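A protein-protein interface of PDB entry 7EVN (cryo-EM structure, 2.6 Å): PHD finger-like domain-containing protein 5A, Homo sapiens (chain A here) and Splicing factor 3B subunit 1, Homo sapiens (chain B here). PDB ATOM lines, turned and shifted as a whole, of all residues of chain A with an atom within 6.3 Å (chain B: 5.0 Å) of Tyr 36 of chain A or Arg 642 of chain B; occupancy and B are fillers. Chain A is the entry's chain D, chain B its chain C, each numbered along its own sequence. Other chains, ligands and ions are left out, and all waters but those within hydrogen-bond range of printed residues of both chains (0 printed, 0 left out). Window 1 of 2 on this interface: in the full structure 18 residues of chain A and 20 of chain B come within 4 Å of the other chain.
O of Ala 636 of chain B lies within hydrogen-bond range of NH1 of Arg 642 of chain B (2.9 Å).
O of Glu 24 of chain A touches O of His 637 of chain B, 3.6 Å away. Lys 639 of chain B touches Asp 27 of chain A. CE2 of Tyr 36 of chain A touches NH2 of Arg 642 of chain B, 3.4 Å away. Arg 643 of chain B touches Tyr 36 of chain A (NH1 to CD2, 3.5 Å).
Of chain B, only Arg 642 (3.4 Å) and Arg 643 (3.5 Å) come within 4 Å of Tyr 36 of chain A. Arg 642 of chain B touches just one residue of chain A: Tyr 36. Printed residues of chain B within 4 Å of Glu 24 of chain A: His 637 (3.6 Å). Of the printed residues of chain A, Lys 639 of chain B touches Asp 27 (3.4 Å). Printed residues of chain A within 4 Å of Arg 643 of chain B: Tyr 36 (3.5 Å). Printed residues of chain B within 4 Å of Asp 27 of chain A: Lys 639 (3.4 Å). Printed residues of chain A within 4 Å of His 637 of chain B: Glu 24 (3.6 Å). The nearest residue of chain A that does not touch Arg 642 of chain B is Gly 28 of chain A (4.2 Å).
Of the 14 printed residues of chain A, 3 touch a printed residue of chain B. Of the 14 printed residues of chain B, 4 touch a printed residue of chain A. Among the printed residues, no Asp or Glu carboxylate lies within 4 Å of a Lys or Arg side-chain nitrogen of the other chain.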
ATOM      1  N   GLU A  24       0.236   6.476 -30.472  1.00  0.00           N
ATOM      2  CA  GLU A  24       0.110   5.161 -29.851  1.00  0.00           C
ATOM      3  C   GLU A  24      -0.293   5.236 -28.385  1.00  0.00           C
ATOM      4  O   GLU A  24      -0.668   4.214 -27.805  1.00  0.00           O
ATOM      5  CB  GLU A  24       1.402   4.363 -30.005  1.00  0.00           C
ATOM      6  CG  GLU A  24       2.548   4.820 -29.139  1.00  0.00           C
ATOM      7  CD  GLU A  24       3.882   4.616 -29.819  1.00  0.00           C
ATOM      8  OE1 GLU A  24       3.902   3.989 -30.897  1.00  0.00           O
ATOM      9  OE2 GLU A  24       4.910   5.064 -29.272  1.00  0.00           O
ATOM     10  N   LYS A  25      -0.212   6.431 -27.795  1.00  0.00           N
ATOM     11  CA  LYS A  25      -0.672   6.619 -26.395  1.00  0.00           C
ATOM     12  C   LYS A  25      -2.201   6.525 -26.418  1.00  0.00           C
ATOM     13  O   LYS A  25      -2.740   5.518 -25.929  1.00  0.00           O
ATOM     14  CB  LYS A  25      -0.231   7.979 -25.847  1.00  0.00           C
ATOM     15  CG  LYS A  25       1.266   8.149 -25.632  1.00  0.00           C
ATOM     16  CD  LYS A  25       1.629   9.501 -25.057  1.00  0.00           C
ATOM     17  CE  LYS A  25       3.086   9.613 -24.661  1.00  0.00           C
ATOM     18  NZ  LYS A  25       3.429   8.690 -23.553  1.00  0.00           N
ATOM     19  N   CYS A  26      -2.862   7.560 -26.948  1.00  0.00           N
ATOM     20  CA  CYS A  26      -4.340   7.566 -27.110  1.00  0.00           C
ATOM     21  C   CYS A  26      -4.646   6.943 -28.472  1.00  0.00           C
ATOM     22  O   CYS A  26      -4.896   7.707 -29.416  1.00  0.00           O
ATOM     23  CB  CYS A  26      -4.881   8.990 -27.066  1.00  0.00           C
ATOM     24  SG  CYS A  26      -3.694  10.248 -27.610  1.00  0.00           S
ATOM     25  N   ASP A  27      -4.671   5.609 -28.542  1.00  0.00           N
ATOM     26  CA  ASP A  27      -4.859   4.879 -29.823  1.00  0.00           C
ATOM     27  C   ASP A  27      -6.303   4.394 -30.002  1.00  0.00           C
ATOM     28  O   ASP A  27      -6.883   4.682 -31.066  1.00  0.00           O
ATOM     29  CB  ASP A  27      -3.864   3.722 -29.928  1.00  0.00           C
ATOM     30  CG  ASP A  27      -4.018   2.909 -31.199  1.00  0.00           C
ATOM     31  OD1 ASP A  27      -4.889   3.260 -32.010  1.00  0.00           O
ATOM     32  OD2 ASP A  27      -3.262   1.936 -31.370  1.00  0.00           O
ATOM     33  N   GLY A  28      -6.868   3.695 -29.014  1.00  0.00           N
ATOM     34  CA  GLY A  28      -8.207   3.167 -29.171  1.00  0.00           C
ATOM     35  C   GLY A  28      -9.313   3.969 -28.521  1.00  0.00           C
ATOM     36  O   GLY A  28     -10.358   3.409 -28.191  1.00  0.00           O
ATOM     37  N   LYS A  29      -9.123   5.270 -28.346  1.00  0.00           N
ATOM     38  CA  LYS A  29     -10.114   6.085 -27.659  1.00  0.00           C
ATOM     39  C   LYS A  29     -11.059   6.761 -28.643  1.00  0.00           C
ATOM     40  O   LYS A  29     -10.754   6.942 -29.820  1.00  0.00           O
ATOM     41  CB  LYS A  29      -9.449   7.156 -26.801  1.00  0.00           C
ATOM     42  CG  LYS A  29      -8.321   6.666 -25.950  1.00  0.00           C
ATOM     43  CD  LYS A  29      -8.129   7.560 -24.742  1.00  0.00           C
ATOM     44  CE  LYS A  29      -7.896   8.992 -25.149  1.00  0.00           C
ATOM     45  NZ  LYS A  29      -8.097   9.920 -24.006  1.00  0.00           N
ATOM     46  N   CYS A  30     -12.219   7.147 -28.126  1.00  0.00           N
ATOM     47  CA  CYS A  30     -13.137   8.003 -28.855  1.00  0.00           C
ATOM     48  C   CYS A  30     -12.677   9.445 -28.728  1.00  0.00           C
ATOM     49  O   CYS A  30     -12.387   9.925 -27.632  1.00  0.00           O
ATOM     50  CB  CYS A  30     -14.557   7.843 -28.312  1.00  0.00           C
ATOM     51  SG  CYS A  30     -15.831   8.813 -29.130  1.00  0.00           S
ATOM     52  N   ASP A  34     -13.676   9.840 -24.864  1.00  0.00           N
ATOM     53  CA  ASP A  34     -12.515   9.211 -24.228  1.00  0.00           C
ATOM     54  C   ASP A  34     -12.763   7.758 -23.837  1.00  0.00           C
ATOM     55  O   ASP A  34     -12.083   7.229 -22.959  1.00  0.00           O
ATOM     56  CB  ASP A  34     -12.054   9.996 -22.996  1.00  0.00           C
ATOM     57  CG  ASP A  34     -10.995  11.019 -23.314  1.00  0.00           C
ATOM     58  OD1 ASP A  34     -10.632  11.172 -24.499  1.00  0.00           O
ATOM     59  OD2 ASP A  34     -10.525  11.679 -22.368  1.00  0.00           O
ATOM     60  N   SER A  35     -13.711   7.091 -24.476  1.00  0.00           N
ATOM     61  CA  SER A  35     -14.078   5.726 -24.137  1.00  0.00           C
ATOM     62  C   SER A  35     -13.311   4.736 -25.005  1.00  0.00           C
ATOM     63  O   SER A  35     -12.771   5.087 -26.053  1.00  0.00           O
ATOM     64  CB  SER A  35     -15.591   5.527 -24.294  1.00  0.00           C
ATOM     65  OG  SER A  35     -15.907   4.230 -24.745  1.00  0.00           O
ATOM     66  N   TYR A  36     -13.261   3.485 -24.548  1.00  0.00           N
ATOM     67  CA  TYR A  36     -12.568   2.417 -25.259  1.00  0.00           C
ATOM     68  C   TYR A  36     -13.512   1.353 -25.793  1.00  0.00           C
ATOM     69  O   TYR A  36     -13.055   0.404 -26.430  1.00  0.00           O
ATOM     70  CB  TYR A  36     -11.525   1.762 -24.358  1.00  0.00           C
ATOM     71  CG  TYR A  36     -10.242   2.534 -24.238  1.00  0.00           C
ATOM     72  CD1 TYR A  36     -10.021   3.382 -23.171  1.00  0.00           C
ATOM     73  CD2 TYR A  36      -9.253   2.413 -25.194  1.00  0.00           C
ATOM     74  CE1 TYR A  36      -8.850   4.089 -23.059  1.00  0.00           C
ATOM     75  CE2 TYR A  36      -8.079   3.113 -25.092  1.00  0.00           C
ATOM     76  CZ  TYR A  36      -7.882   3.948 -24.021  1.00  0.00           C
ATOM     77  OH  TYR A  36      -6.712   4.655 -23.913  1.00  0.00           O
ATOM     78  N   VAL A  37     -14.810   1.485 -25.552  1.00  0.00           N
ATOM     79  CA  VAL A  37     -15.790   0.466 -25.906  1.00  0.00           C
ATOM     80  C   VAL A  37     -16.324   0.753 -27.301  1.00  0.00           C
ATOM     81  O   VAL A  37     -16.803   1.857 -27.574  1.00  0.00           O
ATOM     82  CB  VAL A  37     -16.934   0.422 -24.876  1.00  0.00           C
ATOM     83  CG1 VAL A  37     -17.878  -0.722 -25.172  1.00  0.00           C
ATOM     84  CG2 VAL A  37     -16.377   0.299 -23.477  1.00  0.00           C
ATOM     85  N   ARG A  38     -16.231  -0.243 -28.184  1.00  0.00           N
ATOM     86  CA  ARG A  38     -16.849  -0.285 -29.507  1.00  0.00           C
ATOM     87  C   ARG A  38     -16.544   0.910 -30.408  1.00  0.00           C
ATOM     88  O   ARG A  38     -17.402   1.779 -30.587  1.00  0.00           O
ATOM     89  CB  ARG A  38     -18.362  -0.434 -29.356  1.00  0.00           C
ATOM     90  CG  ARG A  38     -18.810  -1.834 -29.020  1.00  0.00           C
ATOM     91  CD  ARG A  38     -20.304  -1.905 -28.815  1.00  0.00           C
ATOM     92  NE  ARG A  38     -20.702  -3.083 -28.054  1.00  0.00           N
ATOM     93  CZ  ARG A  38     -20.943  -3.080 -26.748  1.00  0.00           C
ATOM     94  NH1 ARG A  38     -20.827  -1.961 -26.055  1.00  0.00           N
ATOM     95  NH2 ARG A  38     -21.302  -4.196 -26.138  1.00  0.00           N
ATOM     96  N   PRO A  39     -15.339   1.002 -30.977  1.00  0.00           N
ATOM     97  CA  PRO A  39     -15.096   1.980 -32.052  1.00  0.00           C
ATOM     98  C   PRO A  39     -15.953   1.681 -33.277  1.00  0.00           C
ATOM     99  O   PRO A  39     -15.902   0.582 -33.827  1.00  0.00           O
ATOM    100  CB  PRO A  39     -13.604   1.800 -32.360  1.00  0.00           C
ATOM    101  CG  PRO A  39     -13.038   1.166 -31.160  1.00  0.00           C
ATOM    102  CD  PRO A  39     -14.108   0.300 -30.590  1.00  0.00           C
ATOM    103  N   CYS A  72     -16.951   6.268 -31.107  1.00  0.00           N
ATOM    104  CA  CYS A  72     -17.511   5.087 -30.471  1.00  0.00           C
ATOM    105  C   CYS A  72     -18.970   4.908 -30.886  1.00  0.00           C
ATOM    106  O   CYS A  72     -19.554   5.740 -31.578  1.00  0.00           O
ATOM    107  CB  CYS A  72     -17.387   5.181 -28.951  1.00  0.00           C
ATOM    108  SG  CYS A  72     -18.397   6.453 -28.177  1.00  0.00           S
ATOM    109  N   LEU B 633      -2.670  -5.957 -16.760  1.00  0.00           N
ATOM    110  CA  LEU B 633      -2.413  -5.644 -18.158  1.00  0.00           C
ATOM    111  C   LEU B 633      -3.660  -5.180 -18.896  1.00  0.00           C
ATOM    112  O   LEU B 633      -3.565  -4.840 -20.079  1.00  0.00           O
ATOM    113  CB  LEU B 633      -1.811  -6.860 -18.862  1.00  0.00           C
ATOM    114  CG  LEU B 633      -0.489  -7.361 -18.283  1.00  0.00           C
ATOM    115  CD1 LEU B 633      -0.135  -8.710 -18.858  1.00  0.00           C
ATOM    116  CD2 LEU B 633       0.617  -6.359 -18.544  1.00  0.00           C
ATOM    117  N   LEU B 634      -4.818  -5.163 -18.237  1.00  0.00           N
ATOM    118  CA  LEU B 634      -6.045  -4.690 -18.865  1.00  0.00           C
ATOM    119  C   LEU B 634      -6.044  -3.192 -19.110  1.00  0.00           C
ATOM    120  O   LEU B 634      -6.890  -2.706 -19.864  1.00  0.00           O
ATOM    121  CB  LEU B 634      -7.253  -5.067 -18.010  1.00  0.00           C
ATOM    122  CG  LEU B 634      -7.505  -6.564 -17.864  1.00  0.00           C
ATOM    123  CD1 LEU B 634      -8.331  -6.844 -16.633  1.00  0.00           C
ATOM    124  CD2 LEU B 634      -8.179  -7.105 -19.108  1.00  0.00           C
ATOM    125  N   LYS B 635      -5.135  -2.453 -18.488  1.00  0.00           N
ATOM    126  CA  LYS B 635      -4.982  -1.030 -18.740  1.00  0.00           C
ATOM    127  C   LYS B 635      -3.618  -0.686 -19.315  1.00  0.00           C
ATOM    128  O   LYS B 635      -3.166   0.450 -19.160  1.00  0.00           O
ATOM    129  CB  LYS B 635      -5.215  -0.240 -17.450  1.00  0.00           C
ATOM    130  CG  LYS B 635      -6.674   0.051 -17.142  1.00  0.00           C
ATOM    131  CD  LYS B 635      -7.286   0.972 -18.178  1.00  0.00           C
ATOM    132  CE  LYS B 635      -8.454   0.324 -18.893  1.00  0.00           C
ATOM    133  NZ  LYS B 635      -9.199   1.333 -19.681  1.00  0.00           N
ATOM    134  N   ALA B 636      -2.951  -1.642 -19.956  1.00  0.00           N
ATOM    135  CA  ALA B 636      -1.629  -1.401 -20.511  1.00  0.00           C
ATOM    136  C   ALA B 636      -1.684  -0.304 -21.564  1.00  0.00           C
ATOM    137  O   ALA B 636      -2.744   0.019 -22.106  1.00  0.00           O
ATOM    138  CB  ALA B 636      -1.064  -2.683 -21.118  1.00  0.00           C
ATOM    139  N   HIS B 637      -0.526   0.275 -21.855  1.00  0.00           N
ATOM    140  CA  HIS B 637      -0.467   1.421 -22.747  1.00  0.00           C
ATOM    141  C   HIS B 637      -0.639   1.064 -24.219  1.00  0.00           C
ATOM    142  O   HIS B 637      -0.908   1.961 -25.021  1.00  0.00           O
ATOM    143  CB  HIS B 637       0.853   2.172 -22.550  1.00  0.00           C
ATOM    144  CG  HIS B 637       0.994   2.796 -21.197  1.00  0.00           C
ATOM    145  ND1 HIS B 637      -0.027   3.499 -20.592  1.00  0.00           N
ATOM    146  CD2 HIS B 637       2.035   2.829 -20.333  1.00  0.00           C
ATOM    147  CE1 HIS B 637       0.379   3.933 -19.413  1.00  0.00           C
ATOM    148  NE2 HIS B 637       1.626   3.540 -19.231  1.00  0.00           N
ATOM    149  N   LYS B 638      -0.510  -0.205 -24.599  1.00  0.00           N
ATOM    150  CA  LYS B 638      -0.571  -0.609 -25.997  1.00  0.00           C
ATOM    151  C   LYS B 638      -1.871  -1.342 -26.307  1.00  0.00           C
ATOM    152  O   LYS B 638      -2.293  -2.233 -25.559  1.00  0.00           O
ATOM    153  CB  LYS B 638       0.624  -1.480 -26.368  1.00  0.00           C
ATOM    154  CG  LYS B 638       1.955  -0.788 -26.173  1.00  0.00           C
ATOM    155  CD  LYS B 638       3.039  -1.363 -27.074  1.00  0.00           C
ATOM    156  CE  LYS B 638       2.796  -1.043 -28.545  1.00  0.00           C
ATOM    157  NZ  LYS B 638       1.876  -1.996 -29.224  1.00  0.00           N
ATOM    158  N   LYS B 639      -2.482  -0.967 -27.432  1.00  0.00           N
ATOM    159  CA  LYS B 639      -3.766  -1.524 -27.835  1.00  0.00           C
ATOM    160  C   LYS B 639      -3.695  -3.026 -28.056  1.00  0.00           C
ATOM    161  O   LYS B 639      -4.643  -3.746 -27.725  1.00  0.00           O
ATOM    162  CB  LYS B 639      -4.248  -0.824 -29.104  1.00  0.00           C
ATOM    163  CG  LYS B 639      -5.741  -0.637 -29.186  1.00  0.00           C
ATOM    164  CD  LYS B 639      -6.287  -1.123 -30.508  1.00  0.00           C
ATOM    165  CE  LYS B 639      -5.886  -0.209 -31.643  1.00  0.00           C
ATOM    166  NZ  LYS B 639      -6.642  -0.508 -32.886  1.00  0.00           N
ATOM    167  N   ALA B 640      -2.584  -3.520 -28.605  1.00  0.00           N
ATOM    168  CA  ALA B 640      -2.466  -4.950 -28.869  1.00  0.00           C
ATOM    169  C   ALA B 640      -2.441  -5.752 -27.574  1.00  0.00           C
ATOM    170  O   ALA B 640      -3.158  -6.752 -27.442  1.00  0.00           O
ATOM    171  CB  ALA B 640      -1.216  -5.231 -29.696  1.00  0.00           C
ATOM    172  N   ILE B 641      -1.628  -5.320 -26.607  1.00  0.00           N
ATOM    173  CA  ILE B 641      -1.593  -5.984 -25.308  1.00  0.00           C
ATOM    174  C   ILE B 641      -2.954  -5.915 -24.637  1.00  0.00           C
ATOM    175  O   ILE B 641      -3.406  -6.888 -24.023  1.00  0.00           O
ATOM    176  CB  ILE B 641      -0.502  -5.366 -24.417  1.00  0.00           C
ATOM    177  CG1 ILE B 641       0.785  -5.160 -25.208  1.00  0.00           C
ATOM    178  CG2 ILE B 641      -0.252  -6.244 -23.211  1.00  0.00           C
ATOM    179  CD1 ILE B 641       1.471  -6.433 -25.575  1.00  0.00           C
ATOM    180  N   ARG B 642      -3.633  -4.770 -24.746  1.00  0.00           N
ATOM    181  CA  ARG B 642      -4.933  -4.632 -24.100  1.00  0.00           C
ATOM    182  C   ARG B 642      -5.954  -5.602 -24.679  1.00  0.00           C
ATOM    183  O   ARG B 642      -6.663  -6.283 -23.928  1.00  0.00           O
ATOM    184  CB  ARG B 642      -5.433  -3.196 -24.222  1.00  0.00           C
ATOM    185  CG  ARG B 642      -4.968  -2.282 -23.116  1.00  0.00           C
ATOM    186  CD  ARG B 642      -5.851  -1.053 -23.029  1.00  0.00           C
ATOM    187  NE  ARG B 642      -6.120  -0.488 -24.345  1.00  0.00           N
ATOM    188  CZ  ARG B 642      -5.387   0.462 -24.910  1.00  0.00           C
ATOM    189  NH1 ARG B 642      -4.339   0.960 -24.279  1.00  0.00           N
ATOM    190  NH2 ARG B 642      -5.706   0.914 -26.108  1.00  0.00           N
ATOM    191  N   ARG B 643      -6.048  -5.684 -26.007  1.00  0.00           N
ATOM    192  CA  ARG B 643      -7.033  -6.575 -26.612  1.00  0.00           C
ATOM    193  C   ARG B 643      -6.690  -8.036 -26.340  1.00  0.00           C
ATOM    194  O   ARG B 643      -7.580  -8.861 -26.083  1.00  0.00           O
ATOM    195  CB  ARG B 643      -7.139  -6.317 -28.113  1.00  0.00           C
ATOM    196  CG  ARG B 643      -7.374  -4.868 -28.510  1.00  0.00           C
ATOM    197  CD  ARG B 643      -8.355  -4.141 -27.594  1.00  0.00           C
ATOM    198  NE  ARG B 643      -8.082  -2.708 -27.542  1.00  0.00           N
ATOM    199  CZ  ARG B 643      -8.564  -1.882 -26.619  1.00  0.00           C
ATOM    200  NH1 ARG B 643      -8.258  -0.592 -26.654  1.00  0.00           N
ATOM    201  NH2 ARG B 643      -9.353  -2.344 -25.658  1.00  0.00           N
ATOM    202  N   ALA B 644      -5.396  -8.374 -26.370  1.00  0.00           N
ATOM    203  CA  ALA B 644      -4.992  -9.743 -26.072  1.00  0.00           C
ATOM    204  C   ALA B 644      -5.356 -10.128 -24.644  1.00  0.00           C
ATOM    205  O   ALA B 644      -5.854 -11.232 -24.400  1.00  0.00           O
ATOM    206  CB  ALA B 644      -3.493  -9.914 -26.305  1.00  0.00           C
ATOM    207  N   THR B 645      -5.128  -9.222 -23.691  1.00  0.00           N
ATOM    208  CA  THR B 645      -5.461  -9.512 -22.303  1.00  0.00           C
ATOM    209  C   THR B 645      -6.964  -9.631 -22.101  1.00  0.00           C
ATOM    210  O   THR B 645      -7.421 -10.491 -21.344  1.00  0.00           O
ATOM    211  CB  THR B 645      -4.884  -8.439 -21.389  1.00  0.00           C
ATOM    212  OG1 THR B 645      -3.504  -8.237 -21.705  1.00  0.00           O
ATOM    213  CG2 THR B 645      -5.002  -8.864 -19.948  1.00  0.00           C
ATOM    214  N   VAL B 646      -7.753  -8.781 -22.763  1.00  0.00           N
ATOM    215  CA  VAL B 646      -9.207  -8.879 -22.638  1.00  0.00           C
ATOM    216  C   VAL B 646      -9.692 -10.239 -23.129  1.00  0.00           C
ATOM    217  O   VAL B 646     -10.480 -10.921 -22.456  1.00  0.00           O
ATOM    218  CB  VAL B 646      -9.894  -7.723 -23.388  1.00  0.00           C
ATOM    219  CG1 VAL B 646     -11.392  -7.914 -23.411  1.00  0.00           C
ATOM    220  CG2 VAL B 646      -9.565  -6.404 -22.735  1.00  0.00           C
